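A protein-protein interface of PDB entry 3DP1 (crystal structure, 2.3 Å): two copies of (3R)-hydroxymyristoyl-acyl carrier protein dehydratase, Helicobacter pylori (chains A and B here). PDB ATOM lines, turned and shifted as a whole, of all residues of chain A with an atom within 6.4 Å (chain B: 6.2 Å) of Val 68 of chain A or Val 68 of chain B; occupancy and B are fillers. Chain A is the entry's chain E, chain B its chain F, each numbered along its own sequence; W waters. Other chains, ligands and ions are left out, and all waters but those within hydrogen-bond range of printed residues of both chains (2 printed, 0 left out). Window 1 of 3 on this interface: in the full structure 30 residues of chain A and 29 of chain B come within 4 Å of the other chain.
Leu 29 of chain A touches none of the printed residues of chain B. Gly 67 of chain A touches none of the printed residues of chain B. Val 68 of chain A touches three residues of chain B. Printed residues of chain A within 4 Å of Pro 66 of chain B: Met 27 (3.5 Å). Of chain A, only Val 68, Glu 72 and Phe 101 come within 4 Å of Val 68 of chain B. Printed residues of chain A within 4 Å of Phe 101 of chain B: Val 68 (3.6 Å) and Phe 109 (3.4 Å). Of the printed residues of chain A, Ile 104 of chain B touches Phe 109 (3.6 Å). Of the printed residues of chain A, Phe 109 of chain B touches Phe 101 and Ile 104. The nearest printed residue of chain B that does not touch Ile 104 of chain A is Val 68 of chain B (4.5 Å).
Met 27 of chain A touches Pro 66 of chain B, and with the chains exchanged Pro 66 of chain A touches Met 27 of chain B. Val 68 of chain A touches Glu 72 of chain B, and with the chains exchanged Glu 72 of chain A touches Val 68 of chain B. Val 68 of chain A touches Phe 101 of chain B, and with the chains exchanged Phe 101 of chain A touches Val 68 of chain B. Phe 101 of chain A touches Phe 109 of chain B, and with the chains exchanged Phe 109 of chain A touches Phe 101 of chain B. Positions printed for both chains: 27, 29, 65, 66, 67, 68, 69, 70, 71, 72, 73, 101, 104 and 109. Of the 11 pairs that touch across the chains among the printed residues, 11 have their exchanged pair printed and touching as well.
Water W2 lies within hydrogen-bond range of the side-chain carboxylate of Glu 72 of chain B (2.6 Å), the backbone NH of Val 68 of chain A (3.0 Å) and the backbone NH of Gly 67 of chain A (3.0 Å). Water W1 lies within hydrogen-bond range of OE2 of Glu 72 of chain A (2.6 Å), N of Val 68 of chain B (3.1 Å) and N of Gly 67 of chain B (3.1 Å).
Of the 14 printed residues of chain A, 7 touch a printed residue of chain B. Printed residues of chain B that touch a printed residue of chain A: Met 27, Pro 66, Val 68, Glu 72, Phe 101, Ile 104 and Phe 109. Hydrophobic or aromatic side chains of chain B that line the printed part of chain A: Met 27, Pro 66, Val 68, Phe 101, Ile 104 and Phe 109. Along chain B the printed residues that touch a printed residue of chain A span positions 27 to 109. Among the printed residues, 11 pairs touch across the chains.
Pro 66 of chain B touches Met 27 of chain A. Pro 66 of chain A touches Met 27 of chain B (CG to CE, 3.7 Å). Val 68 of chain A touches Val 68 of chain B (O to CB, 3.6 Å). Val 68 of chain A touches Glu 72 of chain B (CG1 to OE2, 3.4 Å). Phe 101 of chain B touches Val 68 of chain A. Val 68 of chain B touches Glu 72 of chain A (CG1 to OE2, 3.6 Å). Val 68 of chain B touches Phe 101 of chain A (CG1 to CE2, 3.7 Å). Phe 109 of chain B touches Ile 104 of chain A. Phe 101 of chain B touches Phe 109 of chain A. Ile 104 of chain B touches Phe 109 of chain A (CD1 to CE1, 3.6 Å).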
ATOM      1  N   MET A  27       4.267  -8.825  11.737  1.00  0.00           N
ATOM      2  CA  MET A  27       3.567  -8.063  12.766  1.00  0.00           C
ATOM      3  C   MET A  27       2.199  -7.492  12.387  1.00  0.00           C
ATOM      4  O   MET A  27       1.707  -6.568  13.038  1.00  0.00           O
ATOM      5  CB  MET A  27       4.471  -6.945  13.290  1.00  0.00           C
ATOM      6  CG  MET A  27       5.522  -7.426  14.287  1.00  0.00           C
ATOM      7  SD  MET A  27       4.809  -8.088  15.822  1.00  0.00           S
ATOM      8  CE  MET A  27       4.557  -6.590  16.725  1.00  0.00           C
ATOM      9  N   LEU A  29      -1.244  -8.414  12.624  1.00  0.00           N
ATOM     10  CA  LEU A  29      -2.033  -9.407  13.333  1.00  0.00           C
ATOM     11  C   LEU A  29      -3.559  -9.306  13.254  1.00  0.00           C
ATOM     12  O   LEU A  29      -4.262  -9.712  14.179  1.00  0.00           O
ATOM     13  CB  LEU A  29      -1.573  -9.427  14.800  1.00  0.00           C
ATOM     14  CG  LEU A  29      -0.041  -9.455  14.959  1.00  0.00           C
ATOM     15  CD1 LEU A  29       0.356  -9.564  16.435  1.00  0.00           C
ATOM     16  CD2 LEU A  29       0.528 -10.637  14.168  1.00  0.00           C
ATOM     17  N   PHE A  65      -0.409 -18.974  21.590  1.00  0.00           N
ATOM     18  CA  PHE A  65      -0.274 -17.663  20.976  1.00  0.00           C
ATOM     19  C   PHE A  65       0.077 -16.688  22.098  1.00  0.00           C
ATOM     20  O   PHE A  65      -0.643 -16.583  23.088  1.00  0.00           O
ATOM     21  CB  PHE A  65      -1.572 -17.241  20.283  1.00  0.00           C
ATOM     22  CG  PHE A  65      -1.397 -16.093  19.321  1.00  0.00           C
ATOM     23  CD1 PHE A  65      -0.606 -16.238  18.181  1.00  0.00           C
ATOM     24  CD2 PHE A  65      -2.003 -14.863  19.560  1.00  0.00           C
ATOM     25  CE1 PHE A  65      -0.422 -15.176  17.299  1.00  0.00           C
ATOM     26  CE2 PHE A  65      -1.825 -13.796  18.684  1.00  0.00           C
ATOM     27  CZ  PHE A  65      -1.031 -13.955  17.550  1.00  0.00           C
ATOM     28  N   PRO A  66       1.201 -15.970  21.958  1.00  0.00           N
ATOM     29  CA  PRO A  66       1.627 -15.015  22.988  1.00  0.00           C
ATOM     30  C   PRO A  66       0.552 -13.997  23.376  1.00  0.00           C
ATOM     31  O   PRO A  66      -0.063 -13.370  22.516  1.00  0.00           O
ATOM     32  CB  PRO A  66       2.864 -14.358  22.365  1.00  0.00           C
ATOM     33  CG  PRO A  66       3.414 -15.438  21.465  1.00  0.00           C
ATOM     34  CD  PRO A  66       2.156 -15.995  20.832  1.00  0.00           C
ATOM     35  N   GLY A  67       0.335 -13.858  24.682  1.00  0.00           N
ATOM     36  CA  GLY A  67      -0.644 -12.918  25.195  1.00  0.00           C
ATOM     37  C   GLY A  67      -0.376 -11.500  24.725  1.00  0.00           C
ATOM     38  O   GLY A  67      -1.308 -10.790  24.326  1.00  0.00           O
ATOM     39  N   VAL A  68       0.891 -11.085  24.754  1.00  0.00           N
ATOM     40  CA  VAL A  68       1.244  -9.738  24.317  1.00  0.00           C
ATOM     41  C   VAL A  68       0.897  -9.515  22.845  1.00  0.00           C
ATOM     42  O   VAL A  68       0.652  -8.383  22.428  1.00  0.00           O
ATOM     43  CB  VAL A  68       2.750  -9.412  24.537  1.00  0.00           C
ATOM     44  CG1 VAL A  68       3.117  -9.611  25.988  1.00  0.00           C
ATOM     45  CG2 VAL A  68       3.622 -10.254  23.631  1.00  0.00           C
ATOM     46  N   LEU A  69       0.870 -10.582  22.051  1.00  0.00           N
ATOM     47  CA  LEU A  69       0.528 -10.417  20.646  1.00  0.00           C
ATOM     48  C   LEU A  69      -0.978 -10.271  20.486  1.00  0.00           C
ATOM     49  O   LEU A  69      -1.443  -9.706  19.499  1.00  0.00           O
ATOM     50  CB  LEU A  69       1.057 -11.579  19.796  1.00  0.00           C
ATOM     51  CG  LEU A  69       2.584 -11.622  19.621  1.00  0.00           C
ATOM     52  CD1 LEU A  69       2.945 -12.647  18.558  1.00  0.00           C
ATOM     53  CD2 LEU A  69       3.110 -10.240  19.223  1.00  0.00           C
ATOM     54  N   ILE A  70      -1.732 -10.784  21.458  1.00  0.00           N
ATOM     55  CA  ILE A  70      -3.190 -10.658  21.458  1.00  0.00           C
ATOM     56  C   ILE A  70      -3.477  -9.171  21.679  1.00  0.00           C
ATOM     57  O   ILE A  70      -4.367  -8.589  21.059  1.00  0.00           O
ATOM     58  CB  ILE A  70      -3.827 -11.441  22.622  1.00  0.00           C
ATOM     59  CG1 ILE A  70      -3.636 -12.943  22.417  1.00  0.00           C
ATOM     60  CG2 ILE A  70      -5.308 -11.080  22.742  1.00  0.00           C
ATOM     61  CD1 ILE A  70      -4.049 -13.776  23.614  1.00  0.00           C
ATOM     62  N   VAL A  71      -2.705  -8.570  22.579  1.00  0.00           N
ATOM     63  CA  VAL A  71      -2.846  -7.153  22.879  1.00  0.00           C
ATOM     64  C   VAL A  71      -2.501  -6.349  21.630  1.00  0.00           C
ATOM     65  O   VAL A  71      -3.182  -5.379  21.296  1.00  0.00           O
ATOM     66  CB  VAL A  71      -1.907  -6.732  24.028  1.00  0.00           C
ATOM     67  CG1 VAL A  71      -1.969  -5.220  24.238  1.00  0.00           C
ATOM     68  CG2 VAL A  71      -2.311  -7.449  25.290  1.00  0.00           C
ATOM     69  N   GLU A  72      -1.443  -6.768  20.947  1.00  0.00           N
ATOM     70  CA  GLU A  72      -1.008  -6.106  19.728  1.00  0.00           C
ATOM     71  C   GLU A  72      -2.124  -6.147  18.684  1.00  0.00           C
ATOM     72  O   GLU A  72      -2.361  -5.167  17.987  1.00  0.00           O
ATOM     73  CB  GLU A  72       0.245  -6.792  19.170  1.00  0.00           C
ATOM     74  CG  GLU A  72       0.715  -6.235  17.837  1.00  0.00           C
ATOM     75  CD  GLU A  72       1.242  -4.808  17.940  1.00  0.00           C
ATOM     76  OE1 GLU A  72       1.271  -4.113  16.904  1.00  0.00           O
ATOM     77  OE2 GLU A  72       1.637  -4.385  19.048  1.00  0.00           O
ATOM     78  N   GLY A  73      -2.803  -7.287  18.597  1.00  0.00           N
ATOM     79  CA  GLY A  73      -3.882  -7.451  17.640  1.00  0.00           C
ATOM     80  C   GLY A  73      -5.051  -6.524  17.921  1.00  0.00           C
ATOM     81  O   GLY A  73      -5.666  -5.985  17.003  1.00  0.00           O
ATOM     82  N   PHE A 101       2.312   2.857  20.518  1.00  0.00           N
ATOM     83  CA  PHE A 101       1.611   2.468  21.724  1.00  0.00           C
ATOM     84  C   PHE A 101       1.986   3.539  22.738  1.00  0.00           C
ATOM     85  O   PHE A 101       3.150   3.929  22.837  1.00  0.00           O
ATOM     86  CB  PHE A 101       2.134   1.122  22.224  1.00  0.00           C
ATOM     87  CG  PHE A 101       1.117   0.027  22.202  1.00  0.00           C
ATOM     88  CD1 PHE A 101       0.044   0.041  23.086  1.00  0.00           C
ATOM     89  CD2 PHE A 101       1.248  -1.038  21.317  1.00  0.00           C
ATOM     90  CE1 PHE A 101      -0.885  -0.998  23.094  1.00  0.00           C
ATOM     91  CE2 PHE A 101       0.325  -2.080  21.317  1.00  0.00           C
ATOM     92  CZ  PHE A 101      -0.743  -2.060  22.209  1.00  0.00           C
ATOM     93  N   ILE A 104      -0.896   0.833  28.196  1.00  0.00           N
ATOM     94  CA  ILE A 104      -1.643  -0.419  28.221  1.00  0.00           C
ATOM     95  C   ILE A 104      -2.053  -0.596  29.679  1.00  0.00           C
ATOM     96  O   ILE A 104      -1.227  -0.442  30.573  1.00  0.00           O
ATOM     97  CB  ILE A 104      -0.773  -1.630  27.801  1.00  0.00           C
ATOM     98  CG1 ILE A 104      -0.159  -1.392  26.422  1.00  0.00           C
ATOM     99  CG2 ILE A 104      -1.622  -2.889  27.765  1.00  0.00           C
ATOM    100  CD1 ILE A 104       0.738  -2.517  25.955  1.00  0.00           C
ATOM    101  N   PHE A 109      -5.567 -12.091  31.023  1.00  0.00           N
ATOM    102  CA  PHE A 109      -5.665 -13.215  30.100  1.00  0.00           C
ATOM    103  C   PHE A 109      -6.388 -14.313  30.873  1.00  0.00           C
ATOM    104  O   PHE A 109      -6.003 -14.649  31.987  1.00  0.00           O
ATOM    105  CB  PHE A 109      -4.264 -13.671  29.658  1.00  0.00           C
ATOM    106  CG  PHE A 109      -3.444 -12.579  29.019  1.00  0.00           C
ATOM    107  CD1 PHE A 109      -2.433 -11.938  29.730  1.00  0.00           C
ATOM    108  CD2 PHE A 109      -3.695 -12.181  27.707  1.00  0.00           C
ATOM    109  CE1 PHE A 109      -1.679 -10.913  29.142  1.00  0.00           C
ATOM    110  CE2 PHE A 109      -2.952 -11.161  27.109  1.00  0.00           C
ATOM    111  CZ  PHE A 109      -1.945 -10.526  27.824  1.00  0.00           C
ATOM    112  N   MET B  27      10.956 -15.915  20.195  1.00  0.00           N
ATOM    113  CA  MET B  27      10.287 -15.339  21.352  1.00  0.00           C
ATOM    114  C   MET B  27      11.109 -15.347  22.640  1.00  0.00           C
ATOM    115  O   MET B  27      10.552 -15.167  23.718  1.00  0.00           O
ATOM    116  CB  MET B  27       8.949 -16.046  21.600  1.00  0.00           C
ATOM    117  CG  MET B  27       7.832 -15.600  20.680  1.00  0.00           C
ATOM    118  SD  MET B  27       7.489 -13.829  20.849  1.00  0.00           S
ATOM    119  CE  MET B  27       6.616 -13.787  22.420  1.00  0.00           C
ATOM    120  N   LEU B  29      13.358 -13.245  24.429  1.00  0.00           N
ATOM    121  CA  LEU B  29      13.793 -11.861  24.370  1.00  0.00           C
ATOM    122  C   LEU B  29      14.679 -11.297  25.484  1.00  0.00           C
ATOM    123  O   LEU B  29      14.592 -10.115  25.807  1.00  0.00           O
ATOM    124  CB  LEU B  29      12.551 -10.987  24.174  1.00  0.00           C
ATOM    125  CG  LEU B  29      11.569 -11.541  23.125  1.00  0.00           C
ATOM    126  CD1 LEU B  29      10.399 -10.580  22.949  1.00  0.00           C
ATOM    127  CD2 LEU B  29      12.276 -11.754  21.796  1.00  0.00           C
ATOM    128  N   PHE B  65      11.168  -1.253  17.801  1.00  0.00           N
ATOM    129  CA  PHE B  65      10.993  -2.506  18.533  1.00  0.00           C
ATOM    130  C   PHE B  65       9.615  -2.453  19.191  1.00  0.00           C
ATOM    131  O   PHE B  65       9.339  -1.570  19.997  1.00  0.00           O
ATOM    132  CB  PHE B  65      12.083  -2.670  19.590  1.00  0.00           C
ATOM    133  CG  PHE B  65      12.145  -4.049  20.192  1.00  0.00           C
ATOM    134  CD1 PHE B  65      12.549  -5.144  19.423  1.00  0.00           C
ATOM    135  CD2 PHE B  65      11.798  -4.256  21.524  1.00  0.00           C
ATOM    136  CE1 PHE B  65      12.605  -6.421  19.971  1.00  0.00           C
ATOM    137  CE2 PHE B  65      11.849  -5.528  22.088  1.00  0.00           C
ATOM    138  CZ  PHE B  65      12.254  -6.618  21.311  1.00  0.00           C
ATOM    139  N   PRO B  66       8.732  -3.406  18.853  1.00  0.00           N
ATOM    140  CA  PRO B  66       7.373  -3.457  19.407  1.00  0.00           C
ATOM    141  C   PRO B  66       7.254  -3.261  20.921  1.00  0.00           C
ATOM    142  O   PRO B  66       7.886  -3.965  21.712  1.00  0.00           O
ATOM    143  CB  PRO B  66       6.871  -4.829  18.954  1.00  0.00           C
ATOM    144  CG  PRO B  66       7.572  -5.016  17.636  1.00  0.00           C
ATOM    145  CD  PRO B  66       8.979  -4.561  17.970  1.00  0.00           C
ATOM    146  N   GLY B  67       6.432  -2.291  21.313  1.00  0.00           N
ATOM    147  CA  GLY B  67       6.227  -2.027  22.725  1.00  0.00           C
ATOM    148  C   GLY B  67       5.793  -3.282  23.469  1.00  0.00           C
ATOM    149  O   GLY B  67       6.216  -3.510  24.600  1.00  0.00           O
ATOM    150  N   VAL B  68       4.957  -4.104  22.836  1.00  0.00           N
ATOM    151  CA  VAL B  68       4.492  -5.321  23.482  1.00  0.00           C
ATOM    152  C   VAL B  68       5.629  -6.320  23.716  1.00  0.00           C
ATOM    153  O   VAL B  68       5.579  -7.115  24.661  1.00  0.00           O
ATOM    154  CB  VAL B  68       3.352  -6.002  22.672  1.00  0.00           C
ATOM    155  CG1 VAL B  68       2.155  -5.065  22.574  1.00  0.00           C
ATOM    156  CG2 VAL B  68       3.839  -6.404  21.287  1.00  0.00           C
ATOM    157  N   LEU B  69       6.655  -6.269  22.867  1.00  0.00           N
ATOM    158  CA  LEU B  69       7.802  -7.162  23.007  1.00  0.00           C
ATOM    159  C   LEU B  69       8.744  -6.660  24.102  1.00  0.00           C
ATOM    160  O   LEU B  69       9.525  -7.426  24.661  1.00  0.00           O
ATOM    161  CB  LEU B  69       8.535  -7.309  21.669  1.00  0.00           C
ATOM    162  CG  LEU B  69       7.697  -7.981  20.566  1.00  0.00           C
ATOM    163  CD1 LEU B  69       8.583  -8.276  19.367  1.00  0.00           C
ATOM    164  CD2 LEU B  69       7.061  -9.276  21.091  1.00  0.00           C
ATOM    165  N   ILE B  70       8.667  -5.366  24.405  1.00  0.00           N
ATOM    166  CA  ILE B  70       9.463  -4.795  25.484  1.00  0.00           C
ATOM    167  C   ILE B  70       8.853  -5.389  26.750  1.00  0.00           C
ATOM    168  O   ILE B  70       9.560  -5.853  27.638  1.00  0.00           O
ATOM    169  CB  ILE B  70       9.328  -3.249  25.561  1.00  0.00           C
ATOM    170  CG1 ILE B  70       9.966  -2.600  24.330  1.00  0.00           C
ATOM    171  CG2 ILE B  70       9.988  -2.729  26.844  1.00  0.00           C
ATOM    172  CD1 ILE B  70       9.851  -1.104  24.303  1.00  0.00           C
ATOM    173  N   VAL B  71       7.526  -5.369  26.821  1.00  0.00           N
ATOM    174  CA  VAL B  71       6.822  -5.917  27.973  1.00  0.00           C
ATOM    175  C   VAL B  71       7.095  -7.422  28.097  1.00  0.00           C
ATOM    176  O   VAL B  71       7.283  -7.933  29.198  1.00  0.00           O
ATOM    177  CB  VAL B  71       5.294  -5.675  27.870  1.00  0.00           C
ATOM    178  CG1 VAL B  71       4.566  -6.377  29.017  1.00  0.00           C
ATOM    179  CG2 VAL B  71       5.003  -4.184  27.914  1.00  0.00           C
ATOM    180  N   GLU B  72       7.121  -8.126  26.968  1.00  0.00           N
ATOM    181  CA  GLU B  72       7.391  -9.557  26.979  1.00  0.00           C
ATOM    182  C   GLU B  72       8.774  -9.785  27.584  1.00  0.00           C
ATOM    183  O   GLU B  72       8.958 -10.659  28.431  1.00  0.00           O
ATOM    184  CB  GLU B  72       7.332 -10.128  25.559  1.00  0.00           C
ATOM    185  CG  GLU B  72       7.651 -11.615  25.470  1.00  0.00           C
ATOM    186  CD  GLU B  72       6.591 -12.525  26.107  1.00  0.00           C
ATOM    187  OE1 GLU B  72       6.944 -13.674  26.446  1.00  0.00           O
ATOM    188  OE2 GLU B  72       5.417 -12.113  26.255  1.00  0.00           O
ATOM    189  N   GLY B  73       9.739  -8.979  27.156  1.00  0.00           N
ATOM    190  CA  GLY B  73      11.085  -9.102  27.681  1.00  0.00           C
ATOM    191  C   GLY B  73      11.126  -8.857  29.179  1.00  0.00           C
ATOM    192  O   GLY B  73      11.908  -9.469  29.899  1.00  0.00           O
ATOM    193  N   PHE B 101       1.051 -15.535  30.929  1.00  0.00           N
ATOM    194  CA  PHE B 101       0.829 -14.148  31.294  1.00  0.00           C
ATOM    195  C   PHE B 101      -0.555 -14.150  31.936  1.00  0.00           C
ATOM    196  O   PHE B 101      -1.484 -14.746  31.389  1.00  0.00           O
ATOM    197  CB  PHE B 101       0.803 -13.283  30.034  1.00  0.00           C
ATOM    198  CG  PHE B 101       1.823 -12.188  30.028  1.00  0.00           C
ATOM    199  CD1 PHE B 101       1.705 -11.103  30.887  1.00  0.00           C
ATOM    200  CD2 PHE B 101       2.900 -12.233  29.149  1.00  0.00           C
ATOM    201  CE1 PHE B 101       2.644 -10.076  30.867  1.00  0.00           C
ATOM    202  CE2 PHE B 101       3.839 -11.214  29.123  1.00  0.00           C
ATOM    203  CZ  PHE B 101       3.712 -10.135  29.982  1.00  0.00           C
ATOM    204  N   ILE B 104      -1.480  -7.547  32.985  1.00  0.00           N
ATOM    205  CA  ILE B 104      -0.534  -6.508  32.607  1.00  0.00           C
ATOM    206  C   ILE B 104      -1.221  -5.204  32.981  1.00  0.00           C
ATOM    207  O   ILE B 104      -2.418  -5.042  32.745  1.00  0.00           O
ATOM    208  CB  ILE B 104      -0.279  -6.483  31.089  1.00  0.00           C
ATOM    209  CG1 ILE B 104       0.210  -7.849  30.606  1.00  0.00           C
ATOM    210  CG2 ILE B 104       0.738  -5.410  30.765  1.00  0.00           C
ATOM    211  CD1 ILE B 104       0.341  -7.943  29.094  1.00  0.00           C
ATOM    212  N   PHE B 109       4.849   3.859  27.530  1.00  0.00           N
ATOM    213  CA  PHE B 109       6.044   3.877  26.702  1.00  0.00           C
ATOM    214  C   PHE B 109       6.416   5.341  26.532  1.00  0.00           C
ATOM    215  O   PHE B 109       5.584   6.160  26.156  1.00  0.00           O
ATOM    216  CB  PHE B 109       5.762   3.230  25.349  1.00  0.00           C
ATOM    217  CG  PHE B 109       5.257   1.822  25.455  1.00  0.00           C
ATOM    218  CD1 PHE B 109       3.900   1.541  25.314  1.00  0.00           C
ATOM    219  CD2 PHE B 109       6.140   0.775  25.717  1.00  0.00           C
ATOM    220  CE1 PHE B 109       3.428   0.232  25.431  1.00  0.00           C
ATOM    221  CE2 PHE B 109       5.682  -0.529  25.837  1.00  0.00           C
ATOM    222  CZ  PHE B 109       4.324  -0.806  25.693  1.00  0.00           C
HETATM  223  O   HOH W   1       3.760  -3.313  20.105  1.00  0.00           O
HETATM  224  O   HOH W   2       3.095 -12.951  25.566  1.00  0.00           O
